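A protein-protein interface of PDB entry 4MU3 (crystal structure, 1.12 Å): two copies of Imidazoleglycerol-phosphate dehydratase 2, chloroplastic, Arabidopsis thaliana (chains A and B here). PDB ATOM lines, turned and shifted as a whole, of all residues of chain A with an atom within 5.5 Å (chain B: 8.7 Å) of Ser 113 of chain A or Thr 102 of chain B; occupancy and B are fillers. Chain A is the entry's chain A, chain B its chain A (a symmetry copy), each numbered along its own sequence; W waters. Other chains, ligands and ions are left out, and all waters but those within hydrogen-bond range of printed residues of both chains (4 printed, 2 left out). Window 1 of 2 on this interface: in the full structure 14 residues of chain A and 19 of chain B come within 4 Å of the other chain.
Of the printed residues of chain B, Asp 100 of chain A touches Phe 101 and Thr 102.
No residue of chain B comes within 4 Å of Val 112 of chain A.
Of the printed residues of chain B, Ser 113 of chain A touches Thr 102, Pro 104 and Leu 109.
Of the printed residues of chain A, Thr 102 of chain B touches Asp 100, His 111 and Ser 113.
Of the printed residues of chain A, Ala 108 of chain B touches His 157.
Arg 179 of chain B touches none of the printed residues of chain A.
The nearest printed residue of chain B that does not touch Ser 113 of chain A is Ala 103 of chain B (4.2 Å).
The nearest printed residue of chain A that does not touch Thr 102 of chain B is Gly 99 of chain A (4.7 Å).
The nearest printed residue of chain B that does not touch Thr 155 of chain A is Leu 105 of chain B (4.8 Å).
Asp 100 of chain A touches Phe 101 of chain B, but with the chains exchanged Phe 101 of chain A does not touch Asp 100 of chain B (8.6 Å).
7 positions are printed for both chains.
Of the 13 pairs that touch across the chains among the printed residues, none has its exchanged pair printed and touching as well.
Water W1 bridges OD2 of Asp 115 of chain A and O of Pro 104 of chain B.
Water W4 lies within hydrogen-bond range of OG1 of Thr 155 of chain A (2.6 Å) and OD1 of Asp 106 of chain B (2.7 Å).
Water W3 lies within hydrogen-bond range of the side-chain carboxylate of Asp 100 of chain A (2.7 Å) and the side-chain hydroxyl of Thr 102 of chain B (2.8 Å).
Water W2 lies within hydrogen-bond range of the side-chain hydroxyl (OG1) of Thr 155 of chain A and the backbone NH (N) of Asp 106 of chain B.
Of the 13 printed residues of chain A, 6 touch a printed residue of chain B.
Hydrophobic or aromatic side chains of chain A within 4 Å of the printed part of chain B: His 111 and His 157.
Of the 26 printed residues of chain B, 6 touch a printed residue of chain A.
Among the printed residues, 13 pairs touch across the chains.
Among the printed residues, no Asp or Glu carboxylate lies within 4 Å of a Lys or Arg side-chain nitrogen of the other chain.
Among the printed residues, merely in contact across the chains: Thr 155 of chain A with Asp 106 of chain B (3.4 Å), Ser 113 of chain A with Leu 109 of chain B (3.5 Å), Asp 100 of chain A with Phe 101 of chain B (3.6 Å), Thr 155 of chain A with Pro 104 of chain B (3.7 Å), Ser 113 of chain A with Pro 104 of chain B (3.7 Å), His 111 of chain A with Thr 102 of chain B (3.7 Å), His 157 of chain A with Pro 104 of chain B (3.7 Å), His 157 of chain A with Ala 108 of chain B (3.7 Å), His 157 of chain A with Leu 109 of chain B (3.8 Å) and Asp 115 of chain A with Pro 104 of chain B (3.99 Å).
OD2 of Asp 100 of chain A sits at hydrogen-bond distance from N of Thr 102 of chain B.
The side-chain hydroxyl (OG) of Ser 113 of chain A is in hydrogen-bond range of the backbone carbonyl oxygen (O) of Thr 102 of chain B (3.0 Å).
O of Asp 106 of chain B lies within hydrogen-bond range of NE2 of His 157 of chain A (2.8 Å).
OD1 of Asp 100 of chain A sits at hydrogen-bond distance from NE2 of His 111 of chain A.
The backbone carbonyl oxygen of Ser 113 of chain A lies within hydrogen-bond range of the backbone NH of His 157 of chain A.
The backbone NH of Asp 115 of chain A sits at hydrogen-bond distance from the backbone carbonyl oxygen of Thr 155 of chain A, at 2.9 Å.
O of Phe 101 of chain B sits at hydrogen-bond distance from N of Val 112 of chain B, 2.9 Å away.
N of Leu 161 of chain B lies within hydrogen-bond range of O of Leu 109 of chain B, 2.8 Å away.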
ATOM      1  N   GLY A  99     -21.946  14.556 -20.913  1.00  0.00           N
ATOM      2  CA  GLY A  99     -21.278  13.261 -20.991  1.00  0.00           C
ATOM      3  C   GLY A  99     -20.552  12.931 -19.711  1.00  0.00           C
ATOM      4  O   GLY A  99     -20.086  13.832 -19.016  1.00  0.00           O
ATOM      5  N   ASP A 100     -20.434  11.665 -19.419  1.00  0.00           N
ATOM      6  CA  ASP A 100     -19.884  11.205 -18.153  1.00  0.00           C
ATOM      7  C   ASP A 100     -19.310   9.800 -18.346  1.00  0.00           C
ATOM      8  O   ASP A 100     -20.072   8.886 -18.648  1.00  0.00           O
ATOM      9  CB  ASP A 100     -21.021  11.124 -17.153  1.00  0.00           C
ATOM     10  CG  ASP A 100     -20.545  10.927 -15.764  1.00  0.00           C
ATOM     11  OD1 ASP A 100     -19.457  11.468 -15.464  1.00  0.00           O
ATOM     12  OD2 ASP A 100     -21.262  10.220 -14.996  1.00  0.00           O
ATOM     13  N   PHE A 101     -18.000   9.609 -18.225  1.00  0.00           N
ATOM     14  CA  PHE A 101     -17.454   8.264 -18.361  1.00  0.00           C
ATOM     15  C   PHE A 101     -16.156   8.135 -17.594  1.00  0.00           C
ATOM     16  O   PHE A 101     -15.344   9.059 -17.579  1.00  0.00           O
ATOM     17  CB  PHE A 101     -17.194   7.893 -19.819  1.00  0.00           C
ATOM     18  CG  PHE A 101     -17.185   6.403 -20.034  1.00  0.00           C
ATOM     19  CD1 PHE A 101     -18.361   5.675 -19.945  1.00  0.00           C
ATOM     20  CD2 PHE A 101     -16.012   5.704 -20.228  1.00  0.00           C
ATOM     21  CE1 PHE A 101     -18.364   4.304 -20.057  1.00  0.00           C
ATOM     22  CE2 PHE A 101     -16.022   4.335 -20.347  1.00  0.00           C
ATOM     23  CZ  PHE A 101     -17.202   3.633 -20.268  1.00  0.00           C
ATOM     24  N   HIS A 111     -11.817   9.602 -14.655  1.00  0.00           N
ATOM     25  CA  HIS A 111     -13.206  10.000 -14.774  1.00  0.00           C
ATOM     26  C   HIS A 111     -13.299  11.365 -15.460  1.00  0.00           C
ATOM     27  O   HIS A 111     -12.714  12.333 -14.999  1.00  0.00           O
ATOM     28  CB  HIS A 111     -13.832  10.090 -13.392  1.00  0.00           C
ATOM     29  CG  HIS A 111     -15.231  10.578 -13.395  1.00  0.00           C
ATOM     30  ND1 HIS A 111     -15.756  11.240 -12.330  1.00  0.00           N
ATOM     31  CD2 HIS A 111     -16.235  10.455 -14.291  1.00  0.00           C
ATOM     32  CE1 HIS A 111     -17.019  11.526 -12.575  1.00  0.00           C
ATOM     33  NE2 HIS A 111     -17.323  11.086 -13.781  1.00  0.00           N
ATOM     34  N   VAL A 112     -14.023  11.407 -16.576  1.00  0.00           N
ATOM     35  CA  VAL A 112     -14.315  12.644 -17.280  1.00  0.00           C
ATOM     36  C   VAL A 112     -15.804  12.909 -17.292  1.00  0.00           C
ATOM     37  O   VAL A 112     -16.586  12.063 -17.653  1.00  0.00           O
ATOM     38  CB  VAL A 112     -13.756  12.608 -18.702  1.00  0.00           C
ATOM     39  CG1 VAL A 112     -14.180  13.875 -19.462  1.00  0.00           C
ATOM     40  CG2 VAL A 112     -12.253  12.421 -18.674  1.00  0.00           C
ATOM     41  N   SER A 113     -16.156  14.135 -16.915  1.00  0.00           N
ATOM     42  CA  SER A 113     -17.506  14.626 -16.969  1.00  0.00           C
ATOM     43  C   SER A 113     -17.484  15.962 -17.722  1.00  0.00           C
ATOM     44  O   SER A 113     -16.647  16.816 -17.431  1.00  0.00           O
ATOM     45  CB  SER A 113     -18.007  14.770 -15.522  1.00  0.00           C
ATOM     46  OG  SER A 113     -19.350  15.188 -15.481  1.00  0.00           O
ATOM     47  N   LEU A 114     -18.413  16.162 -18.647  1.00  0.00           N
ATOM     48  CA  LEU A 114     -18.436  17.391 -19.416  1.00  0.00           C
ATOM     49  C   LEU A 114     -19.855  17.805 -19.752  1.00  0.00           C
ATOM     50  O   LEU A 114     -20.775  16.981 -19.820  1.00  0.00           O
ATOM     51  CB  LEU A 114     -17.529  17.295 -20.634  1.00  0.00           C
ATOM     52  CG  LEU A 114     -17.942  16.326 -21.762  1.00  0.00           C
ATOM     53  CD1 LEU A 114     -18.882  17.012 -22.752  1.00  0.00           C
ATOM     54  CD2 LEU A 114     -16.700  15.808 -22.468  1.00  0.00           C
ATOM     55  N   ASP A 115     -19.996  19.095 -20.005  1.00  0.00           N
ATOM     56  CA  ASP A 115     -21.251  19.672 -20.490  1.00  0.00           C
ATOM     57  C   ASP A 115     -20.881  20.640 -21.593  1.00  0.00           C
ATOM     58  O   ASP A 115     -20.052  21.526 -21.421  1.00  0.00           O
ATOM     59  CB  ASP A 115     -22.015  20.379 -19.394  1.00  0.00           C
ATOM     60  CG  ASP A 115     -23.360  20.974 -19.906  1.00  0.00           C
ATOM     61  OD1 ASP A 115     -23.881  20.459 -20.935  1.00  0.00           O
ATOM     62  OD2 ASP A 115     -23.889  21.821 -19.171  1.00  0.00           O
ATOM     63  N   THR A 155     -17.676  22.905 -20.443  1.00  0.00           N
ATOM     64  CA  THR A 155     -17.397  22.621 -19.033  1.00  0.00           C
ATOM     65  C   THR A 155     -16.796  21.222 -18.977  1.00  0.00           C
ATOM     66  O   THR A 155     -17.452  20.268 -19.377  1.00  0.00           O
ATOM     67  CB  THR A 155     -18.695  22.614 -18.209  1.00  0.00           C
ATOM     68  OG1 THR A 155     -19.443  23.813 -18.422  1.00  0.00           O
ATOM     69  CG2 THR A 155     -18.395  22.418 -16.738  1.00  0.00           C
ATOM     70  N   LEU A 156     -15.574  21.080 -18.474  1.00  0.00           N
ATOM     71  CA  LEU A 156     -14.860  19.817 -18.501  1.00  0.00           C
ATOM     72  C   LEU A 156     -14.176  19.560 -17.164  1.00  0.00           C
ATOM     73  O   LEU A 156     -13.414  20.398 -16.712  1.00  0.00           O
ATOM     74  CB  LEU A 156     -13.806  19.861 -19.625  1.00  0.00           C
ATOM     75  CG  LEU A 156     -12.891  18.655 -19.777  1.00  0.00           C
ATOM     76  CD1 LEU A 156     -13.669  17.371 -20.017  1.00  0.00           C
ATOM     77  CD2 LEU A 156     -11.919  18.899 -20.900  1.00  0.00           C
ATOM     78  N   HIS A 157     -14.453  18.404 -16.587  1.00  0.00           N
ATOM     79  CA  HIS A 157     -13.786  17.943 -15.378  1.00  0.00           C
ATOM     80  C   HIS A 157     -13.072  16.624 -15.682  1.00  0.00           C
ATOM     81  O   HIS A 157     -13.664  15.677 -16.205  1.00  0.00           O
ATOM     82  CB  HIS A 157     -14.809  17.710 -14.255  1.00  0.00           C
ATOM     83  CG  HIS A 157     -15.372  18.979 -13.715  1.00  0.00           C
ATOM     84  ND1 HIS A 157     -14.955  19.479 -12.506  1.00  0.00           N
ATOM     85  CD2 HIS A 157     -16.300  19.829 -14.208  1.00  0.00           C
ATOM     86  CE1 HIS A 157     -15.608  20.603 -12.285  1.00  0.00           C
ATOM     87  NE2 HIS A 157     -16.434  20.840 -13.291  1.00  0.00           N
ATOM     88  N   ILE A 158     -11.814  16.565 -15.278  1.00  0.00           N
ATOM     89  CA  ILE A 158     -10.938  15.399 -15.432  1.00  0.00           C
ATOM     90  C   ILE A 158     -10.378  15.032 -14.050  1.00  0.00           C
ATOM     91  O   ILE A 158      -9.694  15.846 -13.451  1.00  0.00           O
ATOM     92  CB  ILE A 158      -9.799  15.701 -16.421  1.00  0.00           C
ATOM     93  CG1 ILE A 158     -10.344  16.023 -17.818  1.00  0.00           C
ATOM     94  CG2 ILE A 158      -8.797  14.556 -16.423  1.00  0.00           C
ATOM     95  CD1 ILE A 158      -9.337  16.466 -18.832  1.00  0.00           C
ATOM     96  N   ALA A 180     -16.969  10.320 -23.193  1.00  0.00           N
ATOM     97  CA  ALA A 180     -17.876  11.347 -22.661  1.00  0.00           C
ATOM     98  C   ALA A 180     -18.336  12.337 -23.741  1.00  0.00           C
ATOM     99  O   ALA A 180     -19.494  12.737 -23.792  1.00  0.00           O
ATOM    100  CB  ALA A 180     -17.199  12.072 -21.501  1.00  0.00           C
ATOM    101  N   GLY B  99     -30.001   4.316 -11.490  1.00  0.00           N
ATOM    102  CA  GLY B  99     -29.474   5.455 -12.236  1.00  0.00           C
ATOM    103  C   GLY B  99     -28.169   5.941 -11.659  1.00  0.00           C
ATOM    104  O   GLY B  99     -27.944   5.827 -10.457  1.00  0.00           O
ATOM    105  N   ASP B 100     -27.335   6.499 -12.495  1.00  0.00           N
ATOM    106  CA  ASP B 100     -25.987   6.886 -12.110  1.00  0.00           C
ATOM    107  C   ASP B 100     -25.516   8.012 -13.032  1.00  0.00           C
ATOM    108  O   ASP B 100     -25.389   7.782 -14.230  1.00  0.00           O
ATOM    109  CB  ASP B 100     -25.081   5.688 -12.316  1.00  0.00           C
ATOM    110  CG  ASP B 100     -23.742   5.875 -11.708  1.00  0.00           C
ATOM    111  OD1 ASP B 100     -23.696   6.547 -10.654  1.00  0.00           O
ATOM    112  OD2 ASP B 100     -22.753   5.358 -12.306  1.00  0.00           O
ATOM    113  N   PHE B 101     -25.295   9.221 -12.523  1.00  0.00           N
ATOM    114  CA  PHE B 101     -24.800  10.285 -13.388  1.00  0.00           C
ATOM    115  C   PHE B 101     -24.031  11.311 -12.585  1.00  0.00           C
ATOM    116  O   PHE B 101     -24.418  11.647 -11.467  1.00  0.00           O
ATOM    117  CB  PHE B 101     -25.930  10.997 -14.129  1.00  0.00           C
ATOM    118  CG  PHE B 101     -25.451  11.664 -15.391  1.00  0.00           C
ATOM    119  CD1 PHE B 101     -25.067  10.902 -16.484  1.00  0.00           C
ATOM    120  CD2 PHE B 101     -25.286  13.031 -15.473  1.00  0.00           C
ATOM    121  CE1 PHE B 101     -24.550  11.487 -17.617  1.00  0.00           C
ATOM    122  CE2 PHE B 101     -24.776  13.610 -16.610  1.00  0.00           C
ATOM    123  CZ  PHE B 101     -24.413  12.837 -17.688  1.00  0.00           C
ATOM    124  N   THR B 102     -22.957  11.836 -13.178  1.00  0.00           N
ATOM    125  CA  THR B 102     -22.198  12.940 -12.643  1.00  0.00           C
ATOM    126  C   THR B 102     -22.313  14.115 -13.604  1.00  0.00           C
ATOM    127  O   THR B 102     -21.980  13.970 -14.769  1.00  0.00           O
ATOM    128  CB  THR B 102     -20.719  12.592 -12.442  1.00  0.00           C
ATOM    129  OG1 THR B 102     -20.594  11.493 -11.528  1.00  0.00           O
ATOM    130  CG2 THR B 102     -19.972  13.746 -11.861  1.00  0.00           C
ATOM    131  N   ALA B 103     -22.855  15.226 -13.090  1.00  0.00           N
ATOM    132  CA  ALA B 103     -23.064  16.441 -13.883  1.00  0.00           C
ATOM    133  C   ALA B 103     -22.349  17.613 -13.268  1.00  0.00           C
ATOM    134  O   ALA B 103     -22.378  17.772 -12.040  1.00  0.00           O
ATOM    135  CB  ALA B 103     -24.516  16.795 -14.004  1.00  0.00           C
ATOM    136  N   PRO B 104     -21.801  18.499 -14.112  1.00  0.00           N
ATOM    137  CA  PRO B 104     -21.239  19.742 -13.613  1.00  0.00           C
ATOM    138  C   PRO B 104     -22.163  20.919 -13.789  1.00  0.00           C
ATOM    139  O   PRO B 104     -23.096  20.901 -14.609  1.00  0.00           O
ATOM    140  CB  PRO B 104     -20.025  19.942 -14.521  1.00  0.00           C
ATOM    141  CG  PRO B 104     -20.475  19.398 -15.845  1.00  0.00           C
ATOM    142  CD  PRO B 104     -21.433  18.274 -15.522  1.00  0.00           C
ATOM    143  N   LEU B 105     -21.841  21.994 -13.079  1.00  0.00           N
ATOM    144  CA  LEU B 105     -22.261  23.354 -13.439  1.00  0.00           C
ATOM    145  C   LEU B 105     -21.012  24.202 -13.167  1.00  0.00           C
ATOM    146  O   LEU B 105     -20.673  24.421 -12.006  1.00  0.00           O
ATOM    147  CB  LEU B 105     -23.488  23.877 -12.691  1.00  0.00           C
ATOM    148  CG  LEU B 105     -24.151  25.048 -13.377  1.00  0.00           C
ATOM    149  CD1 LEU B 105     -25.370  25.525 -12.598  1.00  0.00           C
ATOM    150  CD2 LEU B 105     -23.222  26.213 -13.693  1.00  0.00           C
ATOM    151  N   ASP B 106     -20.295  24.541 -14.219  1.00  0.00           N
ATOM    152  CA  ASP B 106     -19.034  25.257 -14.102  1.00  0.00           C
ATOM    153  C   ASP B 106     -18.106  24.466 -13.184  1.00  0.00           C
ATOM    154  O   ASP B 106     -17.812  23.305 -13.468  1.00  0.00           O
ATOM    155  CB  ASP B 106     -19.225  26.732 -13.747  1.00  0.00           C
ATOM    156  CG  ASP B 106     -19.981  27.522 -14.796  1.00  0.00           C
ATOM    157  OD1 ASP B 106     -20.213  27.011 -15.918  1.00  0.00           O
ATOM    158  OD2 ASP B 106     -20.333  28.677 -14.468  1.00  0.00           O
ATOM    159  N   ALA B 108     -18.618  23.341 -10.190  1.00  0.00           N
ATOM    160  CA  ALA B 108     -19.283  22.326  -9.374  1.00  0.00           C
ATOM    161  C   ALA B 108     -19.443  21.040 -10.155  1.00  0.00           C
ATOM    162  O   ALA B 108     -19.640  21.034 -11.371  1.00  0.00           O
ATOM    163  CB  ALA B 108     -20.632  22.832  -8.911  1.00  0.00           C
ATOM    164  N   LEU B 109     -19.317  19.928  -9.435  1.00  0.00           N
ATOM    165  CA  LEU B 109     -19.412  18.586 -10.030  1.00  0.00           C
ATOM    166  C   LEU B 109     -20.029  17.658  -9.014  1.00  0.00           C
ATOM    167  O   LEU B 109     -19.464  17.489  -7.921  1.00  0.00           O
ATOM    168  CB  LEU B 109     -18.001  18.095 -10.417  1.00  0.00           C
ATOM    169  CG  LEU B 109     -17.979  16.775 -11.206  1.00  0.00           C
ATOM    170  CD1 LEU B 109     -18.559  16.937 -12.600  1.00  0.00           C
ATOM    171  CD2 LEU B 109     -16.569  16.235 -11.288  1.00  0.00           C
ATOM    172  N   ILE B 110     -21.182  17.075  -9.334  1.00  0.00           N
ATOM    173  CA  ILE B 110     -21.955  16.299  -8.376  1.00  0.00           C
ATOM    174  C   ILE B 110     -22.292  14.947  -8.982  1.00  0.00           C
ATOM    175  O   ILE B 110     -22.796  14.869 -10.109  1.00  0.00           O
ATOM    176  CB  ILE B 110     -23.257  17.013  -7.975  1.00  0.00           C
ATOM    177  CG1 ILE B 110     -22.999  18.473  -7.544  1.00  0.00           C
ATOM    178  CG2 ILE B 110     -23.948  16.224  -6.866  1.00  0.00           C
ATOM    179  CD1 ILE B 110     -22.202  18.685  -6.304  1.00  0.00           C
ATOM    180  N   HIS B 111     -21.981  13.880  -8.248  1.00  0.00           N
ATOM    181  CA  HIS B 111     -22.295  12.516  -8.628  1.00  0.00           C
ATOM    182  C   HIS B 111     -23.523  12.031  -7.855  1.00  0.00           C
ATOM    183  O   HIS B 111     -23.536  12.047  -6.634  1.00  0.00           O
ATOM    184  CB  HIS B 111     -21.114  11.613  -8.311  1.00  0.00           C
ATOM    185  CG  HIS B 111     -21.364  10.178  -8.578  1.00  0.00           C
ATOM    186  ND1 HIS B 111     -20.722   9.202  -7.883  1.00  0.00           N
ATOM    187  CD2 HIS B 111     -22.128   9.543  -9.494  1.00  0.00           C
ATOM    188  CE1 HIS B 111     -21.095   8.024  -8.342  1.00  0.00           C
ATOM    189  NE2 HIS B 111     -21.979   8.209  -9.303  1.00  0.00           N
ATOM    190  N   VAL B 112     -24.553  11.626  -8.595  1.00  0.00           N
ATOM    191  CA  VAL B 112     -25.743  11.021  -8.024  1.00  0.00           C
ATOM    192  C   VAL B 112     -25.904   9.598  -8.515  1.00  0.00           C
ATOM    193  O   VAL B 112     -25.860   9.336  -9.692  1.00  0.00           O
ATOM    194  CB  VAL B 112     -26.986  11.851  -8.345  1.00  0.00           C
ATOM    195  CG1 VAL B 112     -28.243  11.130  -7.834  1.00  0.00           C
ATOM    196  CG2 VAL B 112     -26.846  13.249  -7.780  1.00  0.00           C
ATOM    197  N   SER B 113     -26.126   8.700  -7.559  1.00  0.00           N
ATOM    198  CA  SER B 113     -26.422   7.318  -7.822  1.00  0.00           C
ATOM    199  C   SER B 113     -27.695   6.961  -7.045  1.00  0.00           C
ATOM    200  O   SER B 113     -27.803   7.286  -5.863  1.00  0.00           O
ATOM    201  CB  SER B 113     -25.206   6.489  -7.379  1.00  0.00           C
ATOM    202  OG  SER B 113     -25.384   5.122  -7.659  1.00  0.00           O
ATOM    203  N   ARG B 159     -22.921  12.886  -3.965  1.00  0.00           N
ATOM    204  CA  ARG B 159     -21.503  13.117  -3.674  1.00  0.00           C
ATOM    205  C   ARG B 159     -21.034  14.389  -4.349  1.00  0.00           C
ATOM    206  O   ARG B 159     -21.056  14.506  -5.580  1.00  0.00           O
ATOM    207  CB  ARG B 159     -20.634  11.970  -4.182  1.00  0.00           C
ATOM    208  CG  ARG B 159     -20.871  10.642  -3.504  1.00  0.00           C
ATOM    209  CD  ARG B 159     -20.141   9.486  -4.190  1.00  0.00           C
ATOM    210  NE  ARG B 159     -18.678   9.569  -4.199  1.00  0.00           N
ATOM    211  CZ  ARG B 159     -17.878   9.603  -5.274  1.00  0.00           C
ATOM    212  NH1 ARG B 159     -18.314   9.594  -6.542  1.00  0.00           N
ATOM    213  NH2 ARG B 159     -16.575   9.619  -5.043  1.00  0.00           N
ATOM    214  N   GLN B 160     -20.545  15.319  -3.551  1.00  0.00           N
ATOM    215  CA  GLN B 160     -19.943  16.540  -4.046  1.00  0.00           C
ATOM    216  C   GLN B 160     -18.502  16.267  -4.394  1.00  0.00           C
ATOM    217  O   GLN B 160     -17.665  16.012  -3.516  1.00  0.00           O
ATOM    218  CB  GLN B 160     -20.034  17.634  -2.994  1.00  0.00           C
ATOM    219  CG  GLN B 160     -19.457  18.955  -3.442  1.00  0.00           C
ATOM    220  CD  GLN B 160     -19.820  20.091  -2.489  1.00  0.00           C
ATOM    221  OE1 GLN B 160     -20.925  20.094  -1.947  1.00  0.00           O
ATOM    222  NE2 GLN B 160     -18.942  21.065  -2.305  1.00  0.00           N
ATOM    223  N   LEU B 161     -18.186  16.311  -5.681  1.00  0.00           N
ATOM    224  CA  LEU B 161     -16.830  16.051  -6.167  1.00  0.00           C
ATOM    225  C   LEU B 161     -16.006  17.347  -6.291  1.00  0.00           C
ATOM    226  O   LEU B 161     -14.782  17.296  -6.236  1.00  0.00           O
ATOM    227  CB  LEU B 161     -16.846  15.309  -7.494  1.00  0.00           C
ATOM    228  CG  LEU B 161     -17.603  13.983  -7.476  1.00  0.00           C
ATOM    229  CD1 LEU B 161     -17.502  13.326  -8.833  1.00  0.00           C
ATOM    230  CD2 LEU B 161     -17.135  13.064  -6.363  1.00  0.00           C
ATOM    231  N   ALA B 162     -16.686  18.475  -6.512  1.00  0.00           N
ATOM    232  CA  ALA B 162     -16.068  19.782  -6.648  1.00  0.00           C
ATOM    233  C   ALA B 162     -17.175  20.809  -6.502  1.00  0.00           C
ATOM    234  O   ALA B 162     -18.352  20.511  -6.695  1.00  0.00           O
ATOM    235  CB  ALA B 162     -15.395  19.958  -8.014  1.00  0.00           C
ATOM    236  N   ALA B 172     -26.259  21.845  -9.841  1.00  0.00           N
ATOM    237  CA  ALA B 172     -25.606  20.654 -10.414  1.00  0.00           C
ATOM    238  C   ALA B 172     -26.165  19.393  -9.777  1.00  0.00           C
ATOM    239  O   ALA B 172     -26.319  18.372 -10.426  1.00  0.00           O
ATOM    240  CB  ALA B 172     -24.109  20.717 -10.265  1.00  0.00           C
ATOM    241  N   THR B 173     -26.462  19.458  -8.475  1.00  0.00           N
ATOM    242  CA  THR B 173     -27.061  18.309  -7.775  1.00  0.00           C
ATOM    243  C   THR B 173     -28.399  17.954  -8.424  1.00  0.00           C
ATOM    244  O   THR B 173     -28.696  16.785  -8.680  1.00  0.00           O
ATOM    245  CB  THR B 173     -27.248  18.599  -6.283  1.00  0.00           C
ATOM    246  OG1 THR B 173     -25.975  18.820  -5.678  1.00  0.00           O
ATOM    247  CG2 THR B 173     -27.892  17.430  -5.592  1.00  0.00           C
ATOM    248  N   LYS B 175     -29.386  18.684 -11.499  1.00  0.00           N
ATOM    249  CA  LYS B 175     -29.150  18.189 -12.831  1.00  0.00           C
ATOM    250  C   LYS B 175     -28.790  16.703 -12.804  1.00  0.00           C
ATOM    251  O   LYS B 175     -29.301  15.885 -13.579  1.00  0.00           O
ATOM    252  CB  LYS B 175     -28.042  18.954 -13.557  1.00  0.00           C
ATOM    253  CG  LYS B 175     -28.322  20.416 -13.793  1.00  0.00           C
ATOM    254  CD  LYS B 175     -27.125  21.081 -14.520  1.00  0.00           C
ATOM    255  CE  LYS B 175     -27.006  22.556 -14.335  1.00  0.00           C
ATOM    256  NZ  LYS B 175     -28.195  23.275 -14.820  1.00  0.00           N
ATOM    257  N   ALA B 176     -27.859  16.353 -11.931  1.00  0.00           N
ATOM    258  CA  ALA B 176     -27.380  14.981 -11.828  1.00  0.00           C
ATOM    259  C   ALA B 176     -28.480  14.053 -11.339  1.00  0.00           C
ATOM    260  O   ALA B 176     -28.684  12.962 -11.857  1.00  0.00           O
ATOM    261  CB  ALA B 176     -26.163  14.904 -10.925  1.00  0.00           C
ATOM    262  N   PHE B 177     -29.215  14.506 -10.313  1.00  0.00           N
ATOM    263  CA  PHE B 177     -30.348  13.743  -9.794  1.00  0.00           C
ATOM    264  C   PHE B 177     -31.381  13.501 -10.897  1.00  0.00           C
ATOM    265  O   PHE B 177     -31.890  12.399 -11.045  1.00  0.00           O
ATOM    266  CB  PHE B 177     -30.967  14.481  -8.622  1.00  0.00           C
ATOM    267  CG  PHE B 177     -32.254  13.881  -8.121  1.00  0.00           C
ATOM    268  CD1 PHE B 177     -32.263  12.716  -7.363  1.00  0.00           C
ATOM    269  CD2 PHE B 177     -33.463  14.498  -8.379  1.00  0.00           C
ATOM    270  CE1 PHE B 177     -33.440  12.182  -6.883  1.00  0.00           C
ATOM    271  CE2 PHE B 177     -34.648  13.970  -7.887  1.00  0.00           C
ATOM    272  CZ  PHE B 177     -34.631  12.799  -7.146  1.00  0.00           C
ATOM    273  N   ARG B 179     -31.052  13.471 -14.114  1.00  0.00           N
ATOM    274  CA  ARG B 179     -30.545  12.586 -15.161  1.00  0.00           C
ATOM    275  C   ARG B 179     -30.471  11.143 -14.655  1.00  0.00           C
ATOM    276  O   ARG B 179     -30.828  10.206 -15.362  1.00  0.00           O
ATOM    277  CB  ARG B 179     -29.233  13.114 -15.699  1.00  0.00           C
ATOM    278  CG  ARG B 179     -29.478  14.376 -16.531  1.00  0.00           C
ATOM    279  CD  ARG B 179     -28.255  15.224 -16.849  1.00  0.00           C
ATOM    280  NE  ARG B 179     -28.699  16.379 -17.638  1.00  0.00           N
ATOM    281  CZ  ARG B 179     -29.002  16.337 -18.926  1.00  0.00           C
ATOM    282  NH1 ARG B 179     -29.592  17.380 -19.473  1.00  0.00           N
ATOM    283  NH2 ARG B 179     -28.729  15.277 -19.675  1.00  0.00           N
ATOM    284  N   ALA B 180     -30.030  10.965 -13.412  1.00  0.00           N
ATOM    285  CA  ALA B 180     -30.035   9.623 -12.814  1.00  0.00           C
ATOM    286  C   ALA B 180     -31.454   9.055 -12.665  1.00  0.00           C
ATOM    287  O   ALA B 180     -31.703   7.880 -12.909  1.00  0.00           O
ATOM    288  CB  ALA B 180     -29.313   9.662 -11.471  1.00  0.00           C
ATOM    289  N   GLN B 183     -32.803   7.970 -16.033  1.00  0.00           N
ATOM    290  CA  GLN B 183     -32.266   6.663 -16.357  1.00  0.00           C
ATOM    291  C   GLN B 183     -33.029   5.549 -15.598  1.00  0.00           C
ATOM    292  O   GLN B 183     -33.454   4.557 -16.173  1.00  0.00           O
ATOM    293  CB  GLN B 183     -30.776   6.643 -16.037  1.00  0.00           C
ATOM    294  CG  GLN B 183     -30.129   5.297 -16.266  1.00  0.00           C
ATOM    295  CD  GLN B 183     -28.624   5.289 -16.103  1.00  0.00           C
ATOM    296  OE1 GLN B 183     -28.044   6.101 -15.383  1.00  0.00           O
ATOM    297  NE2 GLN B 183     -27.979   4.319 -16.779  1.00  0.00           N
HETATM  298  O   HOH W   1     -23.817  22.525 -16.727  1.00  0.00           O
HETATM  299  O   HOH W   2     -21.679  24.157 -16.807  1.00  0.00           O
HETATM  300  O   HOH W   3     -20.972   8.936 -12.618  1.00  0.00           O
HETATM  301  O   HOH W   4     -18.249  25.900 -17.395  1.00  0.00           O
